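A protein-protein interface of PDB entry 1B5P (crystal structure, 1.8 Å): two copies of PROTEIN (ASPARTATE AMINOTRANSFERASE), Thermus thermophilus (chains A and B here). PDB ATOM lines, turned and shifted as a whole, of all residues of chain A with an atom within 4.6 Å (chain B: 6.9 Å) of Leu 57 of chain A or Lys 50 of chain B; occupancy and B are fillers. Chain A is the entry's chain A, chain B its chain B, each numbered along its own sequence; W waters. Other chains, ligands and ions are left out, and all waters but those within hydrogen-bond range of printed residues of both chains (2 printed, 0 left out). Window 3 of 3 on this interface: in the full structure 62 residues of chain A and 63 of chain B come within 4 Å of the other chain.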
ATOM      1  N   ALA A  53      -9.891 -23.056 -12.417  1.00  0.00           N
ATOM      2  CA  ALA A  53      -8.588 -22.743 -13.005  1.00  0.00           C
ATOM      3  C   ALA A  53      -8.623 -22.924 -14.519  1.00  0.00           C
ATOM      4  O   ALA A  53      -8.111 -22.078 -15.259  1.00  0.00           O
ATOM      5  CB  ALA A  53      -7.499 -23.629 -12.400  1.00  0.00           C
ATOM      6  N   ARG A  54      -9.230 -24.016 -14.982  1.00  0.00           N
ATOM      7  CA  ARG A  54      -9.319 -24.267 -16.418  1.00  0.00           C
ATOM      8  C   ARG A  54     -10.130 -23.184 -17.111  1.00  0.00           C
ATOM      9  O   ARG A  54      -9.802 -22.781 -18.226  1.00  0.00           O
ATOM     10  CB  ARG A  54      -9.944 -25.625 -16.699  1.00  0.00           C
ATOM     11  CG  ARG A  54      -9.061 -26.768 -16.317  1.00  0.00           C
ATOM     12  CD  ARG A  54      -9.831 -28.052 -16.458  1.00  0.00           C
ATOM     13  NE  ARG A  54      -9.156 -29.106 -15.728  1.00  0.00           N
ATOM     14  CZ  ARG A  54      -9.736 -29.884 -14.825  1.00  0.00           C
ATOM     15  NH1 ARG A  54     -11.028 -29.748 -14.532  1.00  0.00           N
ATOM     16  NH2 ARG A  54      -8.992 -30.767 -14.174  1.00  0.00           N
ATOM     17  N   ARG A  55     -11.203 -22.742 -16.463  1.00  0.00           N
ATOM     18  CA  ARG A  55     -12.042 -21.682 -17.012  1.00  0.00           C
ATOM     19  C   ARG A  55     -11.287 -20.373 -17.174  1.00  0.00           C
ATOM     20  O   ARG A  55     -11.460 -19.681 -18.176  1.00  0.00           O
ATOM     21  CB  ARG A  55     -13.253 -21.425 -16.124  1.00  0.00           C
ATOM     22  CG  ARG A  55     -14.254 -22.547 -16.107  1.00  0.00           C
ATOM     23  CD  ARG A  55     -15.651 -21.995 -15.917  1.00  0.00           C
ATOM     24  NE  ARG A  55     -15.804 -21.251 -14.671  1.00  0.00           N
ATOM     25  CZ  ARG A  55     -16.006 -21.819 -13.483  1.00  0.00           C
ATOM     26  NH1 ARG A  55     -16.071 -23.149 -13.381  1.00  0.00           N
ATOM     27  NH2 ARG A  55     -16.177 -21.059 -12.404  1.00  0.00           N
ATOM     28  N   ALA A  56     -10.476 -20.010 -16.174  1.00  0.00           N
ATOM     29  CA  ALA A  56      -9.721 -18.762 -16.255  1.00  0.00           C
ATOM     30  C   ALA A  56      -8.700 -18.850 -17.391  1.00  0.00           C
ATOM     31  O   ALA A  56      -8.487 -17.878 -18.112  1.00  0.00           O
ATOM     32  CB  ALA A  56      -9.042 -18.452 -14.929  1.00  0.00           C
ATOM     33  N   LEU A  57      -8.092 -20.028 -17.547  1.00  0.00           N
ATOM     34  CA  LEU A  57      -7.122 -20.277 -18.609  1.00  0.00           C
ATOM     35  C   LEU A  57      -7.821 -20.085 -19.946  1.00  0.00           C
ATOM     36  O   LEU A  57      -7.339 -19.361 -20.817  1.00  0.00           O
ATOM     37  CB  LEU A  57      -6.590 -21.712 -18.545  1.00  0.00           C
ATOM     38  CG  LEU A  57      -5.401 -22.066 -17.659  1.00  0.00           C
ATOM     39  CD1 LEU A  57      -5.043 -23.531 -17.868  1.00  0.00           C
ATOM     40  CD2 LEU A  57      -4.219 -21.181 -18.013  1.00  0.00           C
ATOM     41  N   ALA A  58      -8.956 -20.763 -20.102  1.00  0.00           N
ATOM     42  CA  ALA A  58      -9.760 -20.681 -21.314  1.00  0.00           C
ATOM     43  C   ALA A  58     -10.219 -19.247 -21.579  1.00  0.00           C
ATOM     44  O   ALA A  58     -10.396 -18.850 -22.730  1.00  0.00           O
ATOM     45  CB  ALA A  58     -10.966 -21.618 -21.208  1.00  0.00           C
ATOM     46  N   GLN A  59     -10.391 -18.471 -20.515  1.00  0.00           N
ATOM     47  CA  GLN A  59     -10.833 -17.081 -20.658  1.00  0.00           C
ATOM     48  C   GLN A  59      -9.745 -16.037 -20.821  1.00  0.00           C
ATOM     49  O   GLN A  59     -10.044 -14.845 -20.892  1.00  0.00           O
ATOM     50  CB  GLN A  59     -11.680 -16.669 -19.479  1.00  0.00           C
ATOM     51  CG  GLN A  59     -13.042 -17.257 -19.500  1.00  0.00           C
ATOM     52  CD  GLN A  59     -13.699 -17.065 -18.181  1.00  0.00           C
ATOM     53  OE1 GLN A  59     -13.033 -17.084 -17.149  1.00  0.00           O
ATOM     54  NE2 GLN A  59     -15.000 -16.847 -18.191  1.00  0.00           N
ATOM     55  N   GLY A  60      -8.494 -16.471 -20.819  1.00  0.00           N
ATOM     56  CA  GLY A  60      -7.400 -15.539 -20.980  1.00  0.00           C
ATOM     57  C   GLY A  60      -7.063 -14.746 -19.737  1.00  0.00           C
ATOM     58  O   GLY A  60      -6.495 -13.655 -19.837  1.00  0.00           O
ATOM     59  N   ILE A 270      -4.351 -16.941 -12.253  1.00  0.00           N
ATOM     60  CA  ILE A 270      -5.097 -18.191 -12.411  1.00  0.00           C
ATOM     61  C   ILE A 270      -5.439 -18.764 -11.030  1.00  0.00           C
ATOM     62  O   ILE A 270      -6.572 -19.165 -10.786  1.00  0.00           O
ATOM     63  CB  ILE A 270      -4.273 -19.237 -13.235  1.00  0.00           C
ATOM     64  CG1 ILE A 270      -3.989 -18.691 -14.658  1.00  0.00           C
ATOM     65  CG2 ILE A 270      -5.027 -20.553 -13.317  1.00  0.00           C
ATOM     66  CD1 ILE A 270      -2.588 -18.137 -14.842  1.00  0.00           C
ATOM     67  N   ASP B  44      -2.398 -13.498 -25.822  1.00  0.00           N
ATOM     68  CA  ASP B  44      -2.683 -14.379 -24.683  1.00  0.00           C
ATOM     69  C   ASP B  44      -1.531 -15.383 -24.640  1.00  0.00           C
ATOM     70  O   ASP B  44      -0.749 -15.466 -25.596  1.00  0.00           O
ATOM     71  CB  ASP B  44      -4.013 -15.111 -24.892  1.00  0.00           C
ATOM     72  CG  ASP B  44      -4.565 -15.746 -23.610  1.00  0.00           C
ATOM     73  OD1 ASP B  44      -3.970 -15.616 -22.516  1.00  0.00           O
ATOM     74  OD2 ASP B  44      -5.641 -16.368 -23.710  1.00  0.00           O
ATOM     75  N   THR B  45      -1.380 -16.109 -23.529  1.00  0.00           N
ATOM     76  CA  THR B  45      -0.289 -17.077 -23.444  1.00  0.00           C
ATOM     77  C   THR B  45      -0.520 -18.220 -24.448  1.00  0.00           C
ATOM     78  O   THR B  45      -1.662 -18.625 -24.709  1.00  0.00           O
ATOM     79  CB  THR B  45       0.097 -17.494 -21.941  1.00  0.00           C
ATOM     80  OG1 THR B  45      -0.016 -18.904 -21.726  1.00  0.00           O
ATOM     81  CG2 THR B  45      -0.744 -16.756 -20.928  1.00  0.00           C
ATOM     82  N   PRO B  46       0.551 -18.604 -25.157  1.00  0.00           N
ATOM     83  CA  PRO B  46       0.447 -19.676 -26.155  1.00  0.00           C
ATOM     84  C   PRO B  46      -0.128 -20.994 -25.640  1.00  0.00           C
ATOM     85  O   PRO B  46       0.128 -21.400 -24.509  1.00  0.00           O
ATOM     86  CB  PRO B  46       1.869 -19.777 -26.715  1.00  0.00           C
ATOM     87  CG  PRO B  46       2.744 -19.136 -25.678  1.00  0.00           C
ATOM     88  CD  PRO B  46       1.906 -18.043 -25.086  1.00  0.00           C
ATOM     89  N   GLU B  47      -0.963 -21.618 -26.461  1.00  0.00           N
ATOM     90  CA  GLU B  47      -1.628 -22.876 -26.105  1.00  0.00           C
ATOM     91  C   GLU B  47      -0.770 -24.022 -25.620  1.00  0.00           C
ATOM     92  O   GLU B  47      -1.253 -24.852 -24.868  1.00  0.00           O
ATOM     93  CB  GLU B  47      -2.492 -23.394 -27.251  1.00  0.00           C
ATOM     94  CG  GLU B  47      -3.791 -22.649 -27.444  1.00  0.00           C
ATOM     95  CD  GLU B  47      -4.776 -22.804 -26.290  1.00  0.00           C
ATOM     96  OE1 GLU B  47      -4.661 -23.763 -25.497  1.00  0.00           O
ATOM     97  OE2 GLU B  47      -5.673 -21.947 -26.200  1.00  0.00           O
ATOM     98  N   HIS B  48       0.468 -24.133 -26.092  1.00  0.00           N
ATOM     99  CA  HIS B  48       1.285 -25.242 -25.616  1.00  0.00           C
ATOM    100  C   HIS B  48       1.569 -25.096 -24.127  1.00  0.00           C
ATOM    101  O   HIS B  48       1.639 -26.097 -23.409  1.00  0.00           O
ATOM    102  CB  HIS B  48       2.570 -25.429 -26.431  1.00  0.00           C
ATOM    103  CG  HIS B  48       3.501 -24.260 -26.400  1.00  0.00           C
ATOM    104  ND1 HIS B  48       4.772 -24.343 -25.891  1.00  0.00           N
ATOM    105  CD2 HIS B  48       3.362 -23.001 -26.882  1.00  0.00           C
ATOM    106  CE1 HIS B  48       5.390 -23.188 -26.062  1.00  0.00           C
ATOM    107  NE2 HIS B  48       4.555 -22.356 -26.664  1.00  0.00           N
ATOM    108  N   VAL B  49       1.678 -23.851 -23.664  1.00  0.00           N
ATOM    109  CA  VAL B  49       1.929 -23.571 -22.253  1.00  0.00           C
ATOM    110  C   VAL B  49       0.620 -23.776 -21.478  1.00  0.00           C
ATOM    111  O   VAL B  49       0.621 -24.421 -20.426  1.00  0.00           O
ATOM    112  CB  VAL B  49       2.559 -22.153 -22.052  1.00  0.00           C
ATOM    113  CG1 VAL B  49       2.657 -21.793 -20.569  1.00  0.00           C
ATOM    114  CG2 VAL B  49       3.958 -22.123 -22.662  1.00  0.00           C
ATOM    115  N   LYS B  50      -0.508 -23.294 -22.024  1.00  0.00           N
ATOM    116  CA  LYS B  50      -1.805 -23.493 -21.361  1.00  0.00           C
ATOM    117  C   LYS B  50      -2.066 -24.998 -21.191  1.00  0.00           C
ATOM    118  O   LYS B  50      -2.442 -25.463 -20.123  1.00  0.00           O
ATOM    119  CB  LYS B  50      -2.954 -22.864 -22.164  1.00  0.00           C
ATOM    120  CG  LYS B  50      -3.041 -21.335 -22.093  1.00  0.00           C
ATOM    121  CD  LYS B  50      -4.323 -20.840 -22.759  1.00  0.00           C
ATOM    122  CE  LYS B  50      -4.496 -19.338 -22.614  1.00  0.00           C
ATOM    123  NZ  LYS B  50      -5.823 -18.947 -23.139  1.00  0.00           N
ATOM    124  N   GLU B  51      -1.817 -25.757 -22.253  1.00  0.00           N
ATOM    125  CA  GLU B  51      -2.004 -27.199 -22.243  1.00  0.00           C
ATOM    126  C   GLU B  51      -1.122 -27.883 -21.193  1.00  0.00           C
ATOM    127  O   GLU B  51      -1.563 -28.824 -20.532  1.00  0.00           O
ATOM    128  CB  GLU B  51      -1.754 -27.765 -23.643  1.00  0.00           C
ATOM    129  CG  GLU B  51      -2.476 -29.069 -23.920  1.00  0.00           C
ATOM    130  CD  GLU B  51      -3.955 -29.019 -23.583  1.00  0.00           C
ATOM    131  OE1 GLU B  51      -4.657 -28.112 -24.077  1.00  0.00           O
ATOM    132  OE2 GLU B  51      -4.414 -29.893 -22.823  1.00  0.00           O
ATOM    133  N   ALA B  52       0.111 -27.418 -21.031  1.00  0.00           N
ATOM    134  CA  ALA B  52       0.989 -28.003 -20.016  1.00  0.00           C
ATOM    135  C   ALA B  52       0.393 -27.754 -18.630  1.00  0.00           C
ATOM    136  O   ALA B  52       0.510 -28.603 -17.745  1.00  0.00           O
ATOM    137  CB  ALA B  52       2.394 -27.423 -20.103  1.00  0.00           C
ATOM    138  N   ALA B  53      -0.244 -26.597 -18.442  1.00  0.00           N
ATOM    139  CA  ALA B  53      -0.890 -26.295 -17.160  1.00  0.00           C
ATOM    140  C   ALA B  53      -2.046 -27.280 -16.934  1.00  0.00           C
ATOM    141  O   ALA B  53      -2.228 -27.791 -15.832  1.00  0.00           O
ATOM    142  CB  ALA B  53      -1.402 -24.859 -17.136  1.00  0.00           C
ATOM    143  N   ARG B  54      -2.801 -27.555 -17.988  1.00  0.00           N
ATOM    144  CA  ARG B  54      -3.911 -28.487 -17.907  1.00  0.00           C
ATOM    145  C   ARG B  54      -3.440 -29.891 -17.518  1.00  0.00           C
ATOM    146  O   ARG B  54      -4.076 -30.548 -16.692  1.00  0.00           O
ATOM    147  CB  ARG B  54      -4.706 -28.492 -19.211  1.00  0.00           C
ATOM    148  CG  ARG B  54      -5.350 -27.155 -19.485  1.00  0.00           C
ATOM    149  CD  ARG B  54      -6.117 -27.165 -20.783  1.00  0.00           C
ATOM    150  NE  ARG B  54      -6.635 -25.837 -21.050  1.00  0.00           N
ATOM    151  CZ  ARG B  54      -6.308 -25.098 -22.105  1.00  0.00           C
ATOM    152  NH1 ARG B  54      -5.456 -25.576 -23.010  1.00  0.00           N
ATOM    153  NH2 ARG B  54      -6.767 -23.849 -22.212  1.00  0.00           N
ATOM    154  N   ARG B  55      -2.314 -30.333 -18.067  1.00  0.00           N
ATOM    155  CA  ARG B  55      -1.781 -31.653 -17.725  1.00  0.00           C
ATOM    156  C   ARG B  55      -1.335 -31.707 -16.264  1.00  0.00           C
ATOM    157  O   ARG B  55      -1.614 -32.691 -15.571  1.00  0.00           O
ATOM    158  CB  ARG B  55      -0.609 -32.041 -18.638  1.00  0.00           C
ATOM    159  CG  ARG B  55      -1.050 -32.465 -20.035  1.00  0.00           C
ATOM    160  CD  ARG B  55       0.058 -33.117 -20.870  1.00  0.00           C
ATOM    161  NE  ARG B  55       1.192 -32.232 -21.148  1.00  0.00           N
ATOM    162  CZ  ARG B  55       1.270 -31.351 -22.146  1.00  0.00           C
ATOM    163  NH1 ARG B  55       0.277 -31.178 -23.018  1.00  0.00           N
ATOM    164  NH2 ARG B  55       2.380 -30.648 -22.277  1.00  0.00           N
ATOM    165  N   LEU B  57      -2.474 -29.983 -13.754  1.00  0.00           N
ATOM    166  CA  LEU B  57      -3.678 -29.996 -12.919  1.00  0.00           C
ATOM    167  C   LEU B  57      -4.205 -31.424 -12.842  1.00  0.00           C
ATOM    168  O   LEU B  57      -4.411 -31.967 -11.755  1.00  0.00           O
ATOM    169  CB  LEU B  57      -4.785 -29.124 -13.517  1.00  0.00           C
ATOM    170  CG  LEU B  57      -4.766 -27.617 -13.331  1.00  0.00           C
ATOM    171  CD1 LEU B  57      -5.978 -27.021 -14.037  1.00  0.00           C
ATOM    172  CD2 LEU B  57      -4.780 -27.270 -11.846  1.00  0.00           C
ATOM    173  N   TRP B 241       1.174 -15.088 -14.705  1.00  0.00           N
ATOM    174  CA  TRP B 241       1.562 -16.393 -14.154  1.00  0.00           C
ATOM    175  C   TRP B 241       2.597 -16.272 -13.044  1.00  0.00           C
ATOM    176  O   TRP B 241       2.779 -17.197 -12.252  1.00  0.00           O
ATOM    177  CB  TRP B 241       2.114 -17.326 -15.229  1.00  0.00           C
ATOM    178  CG  TRP B 241       1.141 -17.702 -16.290  1.00  0.00           C
ATOM    179  CD1 TRP B 241       0.622 -16.874 -17.231  1.00  0.00           C
ATOM    180  CD2 TRP B 241       0.636 -19.013 -16.576  1.00  0.00           C
ATOM    181  NE1 TRP B 241      -0.169 -17.581 -18.094  1.00  0.00           N
ATOM    182  CE2 TRP B 241      -0.182 -18.894 -17.723  1.00  0.00           C
ATOM    183  CE3 TRP B 241       0.786 -20.274 -15.984  1.00  0.00           C
ATOM    184  CZ2 TRP B 241      -0.838 -19.987 -18.295  1.00  0.00           C
ATOM    185  CZ3 TRP B 241       0.131 -21.364 -16.556  1.00  0.00           C
ATOM    186  CH2 TRP B 241      -0.674 -21.207 -17.698  1.00  0.00           C
ATOM    187  N   ILE B 270       1.898 -25.267 -10.529  1.00  0.00           N
ATOM    188  CA  ILE B 270       1.277 -25.434 -11.834  1.00  0.00           C
ATOM    189  C   ILE B 270       1.966 -24.536 -12.874  1.00  0.00           C
ATOM    190  O   ILE B 270       2.198 -24.954 -14.016  1.00  0.00           O
ATOM    191  CB  ILE B 270      -0.225 -25.130 -11.735  1.00  0.00           C
ATOM    192  CG1 ILE B 270      -0.918 -26.161 -10.819  1.00  0.00           C
ATOM    193  CG2 ILE B 270      -0.863 -25.061 -13.122  1.00  0.00           C
ATOM    194  CD1 ILE B 270      -0.667 -25.969  -9.320  1.00  0.00           C
ATOM    195  N   ALA B 274       4.100 -25.379 -16.368  1.00  0.00           N
ATOM    196  CA  ALA B 274       3.724 -24.737 -17.630  1.00  0.00           C
ATOM    197  C   ALA B 274       4.962 -24.065 -18.252  1.00  0.00           C
ATOM    198  O   ALA B 274       5.183 -24.158 -19.457  1.00  0.00           O
ATOM    199  CB  ALA B 274       2.614 -23.707 -17.406  1.00  0.00           C
ATOM    200  N   GLU B 277       7.348 -26.369 -20.093  1.00  0.00           N
ATOM    201  CA  GLU B 277       6.946 -26.600 -21.488  1.00  0.00           C
ATOM    202  C   GLU B 277       7.400 -25.462 -22.423  1.00  0.00           C
ATOM    203  O   GLU B 277       7.822 -25.730 -23.548  1.00  0.00           O
ATOM    204  CB  GLU B 277       5.430 -26.796 -21.600  1.00  0.00           C
ATOM    205  CG  GLU B 277       4.881 -26.884 -23.038  1.00  0.00           C
ATOM    206  CD  GLU B 277       5.204 -28.188 -23.757  1.00  0.00           C
ATOM    207  OE1 GLU B 277       5.792 -29.097 -23.141  1.00  0.00           O
ATOM    208  OE2 GLU B 277       4.851 -28.307 -24.951  1.00  0.00           O
HETATM  209  O   HOH W   1      -8.780 -24.452 -20.035  1.00  0.00           O
HETATM  210  O   HOH W   2      -6.747 -30.362 -16.425  1.00  0.00           O
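NZ of Lys 50 of chain B lies within hydrogen-bond range of O of Leu 57 of chain A, at 2.8 Å.
OD2 of Asp 44 of chain B is in salt-bridge range of NZ of Lys 50 of chain B.
The guanidinium group (NH1) of Arg 54 of chain B lies within salt-bridge range of the side-chain carboxylate (OE1) of Glu 47 of chain B, at 3.2 Å.
The side-chain carboxylate of Glu 51 of chain B is in salt-bridge range of the guanidinium group of Arg 54 of chain B (2.9 Å).
Among the printed residues, pairs that only touch across the chains: Gly 60 of chain A with Asp 44 of chain B, Leu 57 of chain A with Trp 241 of chain B, Ile 270 of chain A with Trp 241 of chain B, Arg 54 of chain A with Leu 57 of chain B, Leu 57 of chain A with Ala 53 of chain B and Leu 57 of chain A with Arg 54 of chain B.
Of the printed residues of chain B, Leu 57 of chain A touches Lys 50, Ala 53, Arg 54 and Trp 241.
Of the printed residues of chain B, Ile 270 of chain A touches Trp 241 (3.8 Å).
Of the printed residues of chain A, Asp 44 of chain B touches Gly 60 (3.4 Å).
Lys 50 of chain B touches one residue of chain A.
Of the printed residues of chain A, Ala 53 of chain B touches Leu 57 (3.9 Å).
Of the printed residues of chain A, Leu 57 of chain B touches Arg 54 (3.8 Å).
The nearest printed residue of chain B that does not touch Leu 57 of chain A is Asp 44 of chain B (4.5 Å).
The nearest residue of chain A that does not touch Lys 50 of chain B is Gly 60 of chain A (4.3 Å).
The nearest printed residue of chain A that does not touch Ala 53 of chain B is Ile 270 of chain A (6.8 Å).
Printed residues of chain A that touch a printed residue of chain B: Arg 54, Leu 57, Gly 60 and Ile 270.
Hydrophobic or aromatic side chains of chain A within 4 Å of the printed part of chain B: Leu 57 and Ile 270.
Arg 54 of chain A touches Leu 57 of chain B, and with the chains exchanged Leu 57 of chain A touches Arg 54 of chain B.
Leu 57 of chain A touches Ala 53 of chain B, but with the chains exchanged Ala 53 of chain A does not touch Leu 57 of chain B (4.1 Å).
Water W1 lies within hydrogen-bond range of O of Arg 54 of chain A (2.7 Å) and NE of Arg 54 of chain B (2.7 Å).
Water W2 lies within hydrogen-bond range of O of Arg 54 of chain B (2.7 Å) and NE of Arg 54 of chain A (2.8 Å).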
